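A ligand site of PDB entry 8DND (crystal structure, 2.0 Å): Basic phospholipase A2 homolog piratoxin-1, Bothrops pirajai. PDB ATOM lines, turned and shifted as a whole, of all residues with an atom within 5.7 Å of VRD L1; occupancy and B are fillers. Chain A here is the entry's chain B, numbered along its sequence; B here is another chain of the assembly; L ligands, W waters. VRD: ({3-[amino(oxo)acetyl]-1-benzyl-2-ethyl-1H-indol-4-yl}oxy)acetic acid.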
ATOM      1  N   LEU A   2      -7.103  31.405  -6.601  1.00  0.00           N
ATOM      2  CA  LEU A   2      -8.081  30.625  -7.342  1.00  0.00           C
ATOM      3  C   LEU A   2      -8.800  31.458  -8.406  1.00  0.00           C
ATOM      4  O   LEU A   2      -9.328  30.887  -9.364  1.00  0.00           O
ATOM      5  CB  LEU A   2      -9.108  30.023  -6.384  1.00  0.00           C
ATOM      6  CG  LEU A   2      -8.628  28.845  -5.518  1.00  0.00           C
ATOM      7  CD1 LEU A   2      -9.742  28.338  -4.623  1.00  0.00           C
ATOM      8  CD2 LEU A   2      -8.091  27.719  -6.391  1.00  0.00           C
ATOM      9  N   PHE A   3      -8.827  32.779  -8.252  1.00  0.00           N
ATOM     10  CA  PHE A   3      -9.386  33.644  -9.285  1.00  0.00           C
ATOM     11  C   PHE A   3      -8.603  33.507 -10.583  1.00  0.00           C
ATOM     12  O   PHE A   3      -9.164  33.224 -11.656  1.00  0.00           O
ATOM     13  CB  PHE A   3      -9.405  35.103  -8.811  1.00  0.00           C
ATOM     14  CG  PHE A   3     -10.063  36.046  -9.787  1.00  0.00           C
ATOM     15  CD1 PHE A   3      -9.355  36.575 -10.850  1.00  0.00           C
ATOM     16  CD2 PHE A   3     -11.388  36.410  -9.630  1.00  0.00           C
ATOM     17  CE1 PHE A   3      -9.957  37.443 -11.742  1.00  0.00           C
ATOM     18  CE2 PHE A   3     -11.997  37.272 -10.512  1.00  0.00           C
ATOM     19  CZ  PHE A   3     -11.288  37.792 -11.570  1.00  0.00           C
ATOM     20  N   LEU A   5      -6.439  31.184 -11.412  1.00  0.00           N
ATOM     21  CA  LEU A   5      -6.469  29.803 -11.882  1.00  0.00           C
ATOM     22  C   LEU A   5      -7.767  29.501 -12.612  1.00  0.00           C
ATOM     23  O   LEU A   5      -7.761  28.907 -13.699  1.00  0.00           O
ATOM     24  CB  LEU A   5      -6.286  28.852 -10.693  1.00  0.00           C
ATOM     25  CG  LEU A   5      -6.499  27.367 -10.965  1.00  0.00           C
ATOM     26  CD1 LEU A   5      -5.506  26.856 -11.998  1.00  0.00           C
ATOM     27  CD2 LEU A   5      -6.395  26.565  -9.676  1.00  0.00           C
ATOM     28  N   GLY A   6      -8.899  29.912 -12.038  1.00  0.00           N
ATOM     29  CA  GLY A   6     -10.175  29.668 -12.686  1.00  0.00           C
ATOM     30  C   GLY A   6     -10.299  30.375 -14.022  1.00  0.00           C
ATOM     31  O   GLY A   6     -10.829  29.821 -14.989  1.00  0.00           O
ATOM     32  N   ILE A   9      -8.198  28.568 -16.659  1.00  0.00           N
ATOM     33  CA  ILE A   9      -8.823  27.328 -17.106  1.00  0.00           C
ATOM     34  C   ILE A   9      -9.934  27.630 -18.100  1.00  0.00           C
ATOM     35  O   ILE A   9     -10.083  26.953 -19.126  1.00  0.00           O
ATOM     36  CB  ILE A   9      -9.337  26.533 -15.892  1.00  0.00           C
ATOM     37  CG1 ILE A   9      -8.174  25.828 -15.193  1.00  0.00           C
ATOM     38  CG2 ILE A   9     -10.402  25.528 -16.317  1.00  0.00           C
ATOM     39  CD1 ILE A   9      -8.490  25.357 -13.789  1.00  0.00           C
ATOM     40  N   PRO A  17     -14.750  26.463 -14.742  1.00  0.00           N
ATOM     41  CA  PRO A  17     -13.800  25.666 -13.965  1.00  0.00           C
ATOM     42  C   PRO A  17     -14.431  24.837 -12.859  1.00  0.00           C
ATOM     43  O   PRO A  17     -14.049  23.672 -12.677  1.00  0.00           O
ATOM     44  CB  PRO A  17     -12.817  26.710 -13.412  1.00  0.00           C
ATOM     45  CG  PRO A  17     -13.392  28.055 -13.739  1.00  0.00           C
ATOM     46  CD  PRO A  17     -14.718  27.899 -14.405  1.00  0.00           C
ATOM     47  N   ALA A  18     -15.377  25.391 -12.095  1.00  0.00           N
ATOM     48  CA  ALA A  18     -15.936  24.629 -10.981  1.00  0.00           C
ATOM     49  C   ALA A  18     -16.864  23.520 -11.473  1.00  0.00           C
ATOM     50  O   ALA A  18     -16.887  22.426 -10.900  1.00  0.00           O
ATOM     51  CB  ALA A  18     -16.675  25.547 -10.016  1.00  0.00           C
ATOM     52  N   TYR A  21     -14.309  20.999 -13.522  1.00  0.00           N
ATOM     53  CA  TYR A  21     -13.075  20.595 -12.868  1.00  0.00           C
ATOM     54  C   TYR A  21     -13.074  20.780 -11.355  1.00  0.00           C
ATOM     55  O   TYR A  21     -12.085  20.420 -10.705  1.00  0.00           O
ATOM     56  CB  TYR A  21     -11.878  21.349 -13.465  1.00  0.00           C
ATOM     57  CG  TYR A  21     -11.653  21.108 -14.929  1.00  0.00           C
ATOM     58  CD1 TYR A  21     -11.193  19.883 -15.400  1.00  0.00           C
ATOM     59  CD2 TYR A  21     -11.884  22.113 -15.859  1.00  0.00           C
ATOM     60  CE1 TYR A  21     -10.985  19.658 -16.746  1.00  0.00           C
ATOM     61  CE2 TYR A  21     -11.669  21.895 -17.215  1.00  0.00           C
ATOM     62  CZ  TYR A  21     -11.223  20.671 -17.641  1.00  0.00           C
ATOM     63  OH  TYR A  21     -11.016  20.455 -18.990  1.00  0.00           O
ATOM     64  N   GLY A  22     -14.148  21.336 -10.776  1.00  0.00           N
ATOM     65  CA  GLY A  22     -14.202  21.501  -9.335  1.00  0.00           C
ATOM     66  C   GLY A  22     -14.079  20.195  -8.563  1.00  0.00           C
ATOM     67  O   GLY A  22     -13.643  20.205  -7.407  1.00  0.00           O
ATOM     68  N   ASN A  27      -7.642  13.929  -8.265  1.00  0.00           N
ATOM     69  CA  ASN A  27      -6.719  15.026  -7.984  1.00  0.00           C
ATOM     70  C   ASN A  27      -7.292  16.417  -8.247  1.00  0.00           C
ATOM     71  O   ASN A  27      -6.756  17.387  -7.693  1.00  0.00           O
ATOM     72  CB  ASN A  27      -5.432  14.871  -8.806  1.00  0.00           C
ATOM     73  CG  ASN A  27      -4.601  13.677  -8.370  1.00  0.00           C
ATOM     74  OD1 ASN A  27      -3.665  13.819  -7.580  1.00  0.00           O
ATOM     75  ND2 ASN A  27      -4.941  12.499  -8.875  1.00  0.00           N
ATOM     76  N   CYS A  28      -8.339  16.555  -9.046  1.00  0.00           N
ATOM     77  CA  CYS A  28      -8.876  17.879  -9.353  1.00  0.00           C
ATOM     78  C   CYS A  28      -9.849  18.319  -8.265  1.00  0.00           C
ATOM     79  O   CYS A  28     -10.772  17.599  -7.905  1.00  0.00           O
ATOM     80  CB  CYS A  28      -9.561  17.870 -10.721  1.00  0.00           C
ATOM     81  SG  CYS A  28      -8.445  17.429 -12.090  1.00  0.00           S
ATOM     82  N   GLY A  29      -9.618  19.521  -7.738  1.00  0.00           N
ATOM     83  CA  GLY A  29     -10.400  20.051  -6.640  1.00  0.00           C
ATOM     84  C   GLY A  29      -9.701  19.893  -5.311  1.00  0.00           C
ATOM     85  O   GLY A  29      -8.508  19.577  -5.227  1.00  0.00           O
ATOM     86  N   VAL A  30     -10.470  20.131  -4.250  1.00  0.00           N
ATOM     87  CA  VAL A  30      -9.932  19.953  -2.909  1.00  0.00           C
ATOM     88  C   VAL A  30      -9.791  18.460  -2.598  1.00  0.00           C
ATOM     89  O   VAL A  30     -10.286  17.596  -3.342  1.00  0.00           O
ATOM     90  CB  VAL A  30     -10.808  20.659  -1.870  1.00  0.00           C
ATOM     91  CG1 VAL A  30     -11.024  22.118  -2.256  1.00  0.00           C
ATOM     92  CG2 VAL A  30     -12.150  19.951  -1.738  1.00  0.00           C
ATOM     93  N   GLY A  32      -6.625  16.948  -1.802  1.00  0.00           N
ATOM     94  CA  GLY A  32      -5.286  16.441  -1.994  1.00  0.00           C
ATOM     95  C   GLY A  32      -5.126  15.566  -3.228  1.00  0.00           C
ATOM     96  O   GLY A  32      -5.953  15.552  -4.136  1.00  0.00           O
ATOM     97  N   CYS A  43      -3.147  16.069 -14.786  1.00  0.00           N
ATOM     98  CA  CYS A  43      -2.865  17.502 -14.812  1.00  0.00           C
ATOM     99  C   CYS A  43      -2.972  18.096 -13.410  1.00  0.00           C
ATOM    100  O   CYS A  43      -2.095  18.834 -12.964  1.00  0.00           O
ATOM    101  CB  CYS A  43      -3.821  18.214 -15.768  1.00  0.00           C
ATOM    102  SG  CYS A  43      -3.780  17.649 -17.486  1.00  0.00           S
ATOM    103  N   CYS A  44      -4.059  17.773 -12.708  1.00  0.00           N
ATOM    104  CA  CYS A  44      -4.250  18.278 -11.351  1.00  0.00           C
ATOM    105  C   CYS A  44      -3.265  17.646 -10.380  1.00  0.00           C
ATOM    106  O   CYS A  44      -2.884  18.273  -9.379  1.00  0.00           O
ATOM    107  CB  CYS A  44      -5.691  18.025 -10.904  1.00  0.00           C
ATOM    108  SG  CYS A  44      -6.936  18.792 -11.984  1.00  0.00           S
ATOM    109  N   TYR A  45      -2.847  16.407 -10.638  1.00  0.00           N
ATOM    110  CA  TYR A  45      -1.798  15.774  -9.848  1.00  0.00           C
ATOM    111  C   TYR A  45      -0.492  16.566  -9.946  1.00  0.00           C
ATOM    112  O   TYR A  45       0.097  16.937  -8.927  1.00  0.00           O
ATOM    113  CB  TYR A  45      -1.609  14.329 -10.304  1.00  0.00           C
ATOM    114  CG  TYR A  45      -0.557  13.505  -9.573  1.00  0.00           C
ATOM    115  CD1 TYR A  45       0.802  13.714  -9.791  1.00  0.00           C
ATOM    116  CD2 TYR A  45      -0.930  12.504  -8.683  1.00  0.00           C
ATOM    117  CE1 TYR A  45       1.756  12.963  -9.143  1.00  0.00           C
ATOM    118  CE2 TYR A  45       0.024  11.744  -8.030  1.00  0.00           C
ATOM    119  CZ  TYR A  45       1.359  11.980  -8.257  1.00  0.00           C
ATOM    120  OH  TYR A  45       2.307  11.223  -7.598  1.00  0.00           O
ATOM    121  N   HIS A  47      -0.180  19.581 -10.956  1.00  0.00           N
ATOM    122  CA  HIS A  47      -0.438  20.928 -10.458  1.00  0.00           C
ATOM    123  C   HIS A  47      -0.214  21.003  -8.956  1.00  0.00           C
ATOM    124  O   HIS A  47       0.395  21.953  -8.452  1.00  0.00           O
ATOM    125  CB  HIS A  47      -1.859  21.346 -10.824  1.00  0.00           C
ATOM    126  CG  HIS A  47      -2.173  22.769 -10.474  1.00  0.00           C
ATOM    127  ND1 HIS A  47      -3.251  23.122  -9.699  1.00  0.00           N
ATOM    128  CD2 HIS A  47      -1.559  23.922 -10.824  1.00  0.00           C
ATOM    129  CE1 HIS A  47      -3.285  24.441  -9.568  1.00  0.00           C
ATOM    130  NE2 HIS A  47      -2.271  24.945 -10.241  1.00  0.00           N
ATOM    131  N   LYS A  48      -0.709  20.013  -8.214  1.00  0.00           N
ATOM    132  CA  LYS A  48      -0.544  20.034  -6.758  1.00  0.00           C
ATOM    133  C   LYS A  48       0.910  19.810  -6.357  1.00  0.00           C
ATOM    134  O   LYS A  48       1.380  20.390  -5.375  1.00  0.00           O
ATOM    135  CB  LYS A  48      -1.451  18.975  -6.121  1.00  0.00           C
ATOM    136  CG  LYS A  48      -2.873  19.464  -5.907  1.00  0.00           C
ATOM    137  CD  LYS A  48      -3.834  18.309  -5.695  1.00  0.00           C
ATOM    138  CE  LYS A  48      -5.238  18.827  -5.408  1.00  0.00           C
ATOM    139  NZ  LYS A  48      -6.231  17.719  -5.270  1.00  0.00           N
ATOM    140  N   TYR A  51       2.519  23.149  -6.744  1.00  0.00           N
ATOM    141  CA  TYR A  51       2.247  23.998  -5.581  1.00  0.00           C
ATOM    142  C   TYR A  51       3.162  23.666  -4.421  1.00  0.00           C
ATOM    143  O   TYR A  51       3.576  24.559  -3.672  1.00  0.00           O
ATOM    144  CB  TYR A  51       0.783  23.853  -5.162  1.00  0.00           C
ATOM    145  CG  TYR A  51      -0.190  24.735  -5.904  1.00  0.00           C
ATOM    146  CD1 TYR A  51       0.212  25.504  -6.998  1.00  0.00           C
ATOM    147  CD2 TYR A  51      -1.524  24.800  -5.517  1.00  0.00           C
ATOM    148  CE1 TYR A  51      -0.689  26.305  -7.669  1.00  0.00           C
ATOM    149  CE2 TYR A  51      -2.426  25.601  -6.189  1.00  0.00           C
ATOM    150  CZ  TYR A  51      -2.009  26.361  -7.261  1.00  0.00           C
ATOM    151  OH  TYR A  51      -2.909  27.152  -7.928  1.00  0.00           O
ATOM    152  N   PRO A  59      -0.802  29.762  -2.539  1.00  0.00           N
ATOM    153  CA  PRO A  59      -1.412  29.564  -3.868  1.00  0.00           C
ATOM    154  C   PRO A  59      -2.890  29.890  -3.907  1.00  0.00           C
ATOM    155  O   PRO A  59      -3.411  30.262  -4.973  1.00  0.00           O
ATOM    156  CB  PRO A  59      -1.150  28.079  -4.155  1.00  0.00           C
ATOM    157  CG  PRO A  59      -0.098  27.650  -3.177  1.00  0.00           C
ATOM    158  CD  PRO A  59      -0.292  28.505  -1.974  1.00  0.00           C
ATOM    159  N   LYS A  60      -3.599  29.770  -2.781  1.00  0.00           N
ATOM    160  CA  LYS A  60      -5.049  29.945  -2.787  1.00  0.00           C
ATOM    161  C   LYS A  60      -5.452  31.410  -2.704  1.00  0.00           C
ATOM    162  O   LYS A  60      -6.425  31.826  -3.359  1.00  0.00           O
ATOM    163  CB  LYS A  60      -5.677  29.164  -1.634  1.00  0.00           C
ATOM    164  CG  LYS A  60      -5.386  27.673  -1.661  1.00  0.00           C
ATOM    165  CD  LYS A  60      -5.790  27.066  -3.002  1.00  0.00           C
ATOM    166  CE  LYS A  60      -5.888  25.553  -2.900  1.00  0.00           C
ATOM    167  NZ  LYS A  60      -6.724  25.114  -1.755  1.00  0.00           N
ATOM    168  N   VAL A  92      -1.302  23.880 -15.678  1.00  0.00           N
ATOM    169  CA  VAL A  92      -2.458  22.998 -15.540  1.00  0.00           C
ATOM    170  C   VAL A  92      -3.565  23.411 -16.497  1.00  0.00           C
ATOM    171  O   VAL A  92      -4.289  22.564 -17.022  1.00  0.00           O
ATOM    172  CB  VAL A  92      -2.934  22.965 -14.080  1.00  0.00           C
ATOM    173  CG1 VAL A  92      -3.593  24.274 -13.671  1.00  0.00           C
ATOM    174  CG2 VAL A  92      -3.894  21.792 -13.858  1.00  0.00           C
ATOM    175  N   LEU A  96      -5.034  20.727 -19.073  1.00  0.00           N
ATOM    176  CA  LEU A  96      -6.441  20.350 -19.160  1.00  0.00           C
ATOM    177  C   LEU A  96      -6.982  20.561 -20.566  1.00  0.00           C
ATOM    178  O   LEU A  96      -7.766  19.750 -21.080  1.00  0.00           O
ATOM    179  CB  LEU A  96      -7.266  21.130 -18.141  1.00  0.00           C
ATOM    180  CG  LEU A  96      -6.939  20.924 -16.669  1.00  0.00           C
ATOM    181  CD1 LEU A  96      -7.686  21.937 -15.802  1.00  0.00           C
ATOM    182  CD2 LEU A  96      -7.252  19.502 -16.233  1.00  0.00           C
ATOM    183  N   VAL B  30     -15.347  27.388  -2.790  1.00  0.00           N
ATOM    184  CA  VAL B  30     -14.172  28.218  -3.028  1.00  0.00           C
ATOM    185  C   VAL B  30     -14.498  29.692  -2.794  1.00  0.00           C
ATOM    186  O   VAL B  30     -15.657  30.111  -2.754  1.00  0.00           O
ATOM    187  CB  VAL B  30     -13.637  27.992  -4.452  1.00  0.00           C
ATOM    188  CG1 VAL B  30     -13.022  26.614  -4.578  1.00  0.00           C
ATOM    189  CG2 VAL B  30     -14.759  28.176  -5.472  1.00  0.00           C
ATOM    190  N   LEU B  31     -13.441  30.485  -2.593  1.00  0.00           N
ATOM    191  CA  LEU B  31     -13.459  31.943  -2.759  1.00  0.00           C
ATOM    192  C   LEU B  31     -14.201  32.663  -1.632  1.00  0.00           C
ATOM    193  O   LEU B  31     -14.920  33.631  -1.871  1.00  0.00           O
ATOM    194  CB  LEU B  31     -14.036  32.322  -4.121  1.00  0.00           C
ATOM    195  CG  LEU B  31     -13.229  31.832  -5.318  1.00  0.00           C
ATOM    196  CD1 LEU B  31     -13.910  32.251  -6.609  1.00  0.00           C
ATOM    197  CD2 LEU B  31     -11.800  32.352  -5.265  1.00  0.00           C
HETATM  198  C01 VRD L   1      -8.891  21.961 -11.820  1.00  0.00           C
HETATM  199  C02 VRD L   1      -9.642  23.020 -10.994  1.00  0.00           C
HETATM  200  C03 VRD L   1      -9.268  23.157  -9.484  1.00  0.00           C
HETATM  201  C04 VRD L   1      -8.037  22.875  -8.856  1.00  0.00           C
HETATM  202  C05 VRD L   1      -8.224  23.181  -7.489  1.00  0.00           C
HETATM  203  C06 VRD L   1      -9.529  23.625  -7.358  1.00  0.00           C
HETATM  204  C08 VRD L   1     -11.504  24.003  -8.829  1.00  0.00           C
HETATM  205  C09 VRD L   1     -11.604  25.507  -9.192  1.00  0.00           C
HETATM  206  C10 VRD L   1     -10.467  26.283  -9.291  1.00  0.00           C
HETATM  207  C11 VRD L   1     -10.567  27.634  -9.621  1.00  0.00           C
HETATM  208  C12 VRD L   1     -11.810  28.195  -9.854  1.00  0.00           C
HETATM  209  C13 VRD L   1     -12.954  27.415  -9.762  1.00  0.00           C
HETATM  210  C14 VRD L   1     -12.854  26.064  -9.432  1.00  0.00           C
HETATM  211  C15 VRD L   1     -10.028  24.012  -6.106  1.00  0.00           C
HETATM  212  C16 VRD L   1      -9.209  23.949  -4.981  1.00  0.00           C
HETATM  213  C17 VRD L   1      -7.890  23.498  -5.107  1.00  0.00           C
HETATM  214  C18 VRD L   1      -7.398  23.113  -6.352  1.00  0.00           C
HETATM  215  C20 VRD L   1      -5.101  23.453  -5.824  1.00  0.00           C
HETATM  216  C21 VRD L   1      -4.740  22.801  -4.489  1.00  0.00           C
HETATM  217  C24 VRD L   1      -6.731  22.341  -9.475  1.00  0.00           C
HETATM  218  C26 VRD L   1      -6.062  21.061  -8.938  1.00  0.00           C
HETATM  219  N07 VRD L   1     -10.113  23.605  -8.571  1.00  0.00           N
HETATM  220  N28 VRD L   1      -6.830  20.107  -8.149  1.00  0.00           N
HETATM  221  O19 VRD L   1      -6.057  22.658  -6.468  1.00  0.00           O
HETATM  222  O22 VRD L   1      -5.206  21.664  -4.197  1.00  0.00           O
HETATM  223  O23 VRD L   1      -3.978  23.383  -3.678  1.00  0.00           O
HETATM  224  O25 VRD L   1      -6.227  22.922 -10.384  1.00  0.00           O
HETATM  225  O27 VRD L   1      -4.929  20.858  -9.165  1.00  0.00           O
HETATM  226  C01 VRD L   2     -13.086  33.439  -9.860  1.00  0.00           C
HETATM  227  C02 VRD L   2     -12.888  32.047 -10.473  1.00  0.00           C
HETATM  228  C03 VRD L   2     -13.983  31.711 -11.512  1.00  0.00           C
HETATM  229  C04 VRD L   2     -15.145  30.967 -11.264  1.00  0.00           C
HETATM  230  C05 VRD L   2     -15.848  30.918 -12.491  1.00  0.00           C
HETATM  231  C06 VRD L   2     -15.085  31.623 -13.405  1.00  0.00           C
HETATM  232  C08 VRD L   2     -12.942  32.894 -13.427  1.00  0.00           C
HETATM  233  C09 VRD L   2     -13.492  34.346 -13.578  1.00  0.00           C
HETATM  234  C10 VRD L   2     -14.677  34.713 -12.951  1.00  0.00           C
HETATM  235  C11 VRD L   2     -15.169  35.996 -13.088  1.00  0.00           C
HETATM  236  C12 VRD L   2     -14.484  36.923 -13.851  1.00  0.00           C
HETATM  237  C13 VRD L   2     -13.300  36.564 -14.482  1.00  0.00           C
HETATM  238  C14 VRD L   2     -12.801  35.279 -14.351  1.00  0.00           C
HETATM  239  C15 VRD L   2     -15.507  31.769 -14.738  1.00  0.00           C
HETATM  240  C16 VRD L   2     -16.704  31.201 -15.154  1.00  0.00           C
HETATM  241  C17 VRD L   2     -17.479  30.479 -14.249  1.00  0.00           C
HETATM  242  C18 VRD L   2     -17.065  30.337 -12.926  1.00  0.00           C
HETATM  243  C20 VRD L   2     -17.469  28.262 -11.932  1.00  0.00           C
HETATM  244  C21 VRD L   2     -18.326  27.399 -12.847  1.00  0.00           C
HETATM  245  C24 VRD L   2     -15.540  30.351  -9.906  1.00  0.00           C
HETATM  246  C26 VRD L   2     -16.947  30.579  -9.353  1.00  0.00           C
HETATM  247  N07 VRD L   2     -13.986  32.086 -12.786  1.00  0.00           N
HETATM  248  N28 VRD L   2     -17.574  31.870  -9.558  1.00  0.00           N
HETATM  249  O19 VRD L   2     -17.875  29.609 -12.027  1.00  0.00           O
HETATM  250  O22 VRD L   2     -17.978  26.226 -13.119  1.00  0.00           O
HETATM  251  O23 VRD L   2     -19.396  27.864 -13.332  1.00  0.00           O
HETATM  252  O25 VRD L   2     -14.754  29.726  -9.270  1.00  0.00           O
HETATM  253  O27 VRD L   2     -17.516  29.716  -8.787  1.00  0.00           O
HETATM  254  O   HOH W   1     -13.297  22.630  -6.274  1.00  0.00           O
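An oxygen (O23) of VRD L1 is in salt-bridge range of the side-chain amino group of Lys 60 (3.8 Å). An oxygen (O27) of VRD L1 lies within hydrogen-bond range of a ring nitrogen (ND1) of His 47 (2.9 Å). O22 of VRD L2 lies within hydrogen-bond range of N of Ala 18, 2.9 Å away. N28 of VRD L1 lies within hydrogen-bond range of O of Asn 27, 2.8 Å away. A nitrogen (N28) of VRD L1 lies within hydrogen-bond range of the backbone carbonyl oxygen (O) of Gly 29.
N of Gly 22 lies within hydrogen-bond range of O of Pro 17 (3.0 Å). SG of Cys 44 forms a disulfide with SG of Cys 28 (2.0 Å). OH of Tyr 51 sits close to NE2 of His 47 (3.3 Å). The backbone carbonyl oxygen (O) of Lys 60 sits at hydrogen-bond distance from the backbone NH (N) of Leu 2, 3.3 Å away. The side-chain amino group (NZ) of Lys 48 is in hydrogen-bond range of the backbone carbonyl oxygen (O) of Asn 27 (2.5 Å). The backbone carbonyl oxygen (O) of Gly 29 sits at hydrogen-bond distance from the side-chain amino group (NZ) of Lys 48, at 2.9 Å. The side-chain amino group of Lys 48 sits at hydrogen-bond distance from the backbone carbonyl oxygen of Gly 32, at 2.5 Å.
O of Cys 44 sits close to O27 of VRD L1, 3.3 Å away. Residues that only touch VRD L1: Leu 2 (3.5 Å), Leu 5 (3.7 Å), Gly 6 (3.6 Å), Ile 9 (3.8 Å), Pro 17 (3.7 Å), Ala 18 (3.7 Å), Tyr 21 (3.5 Å), Gly 22 (3.7 Å), Cys 28 (3.3 Å), Val 30 of chain A (3.8 Å), Lys 48 (3.1 Å) and Tyr 51 (3.4 Å). Hydrophobic or aromatic side chains that line VRD L1: Leu 5, Ile 9, Pro 17, Ala 18, Tyr 21, Val 30 of chain A, His 47 and Tyr 51. 17 residues have an atom within 4 Å of VRD L1: Leu 2, Leu 5, Gly 6, Ile 9, Pro 17, Ala 18, Tyr 21, Gly 22, Asn 27, Cys 28, Gly 29, Val 30 of chain A, Cys 44, His 47, Lys 48, Tyr 51 and Lys 60. Along chain A the residues within 4 Å of VRD L1 span positions 2 to 60. The nearest printed residue that does not touch VRD L1 is Leu 96 (4.2 Å).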
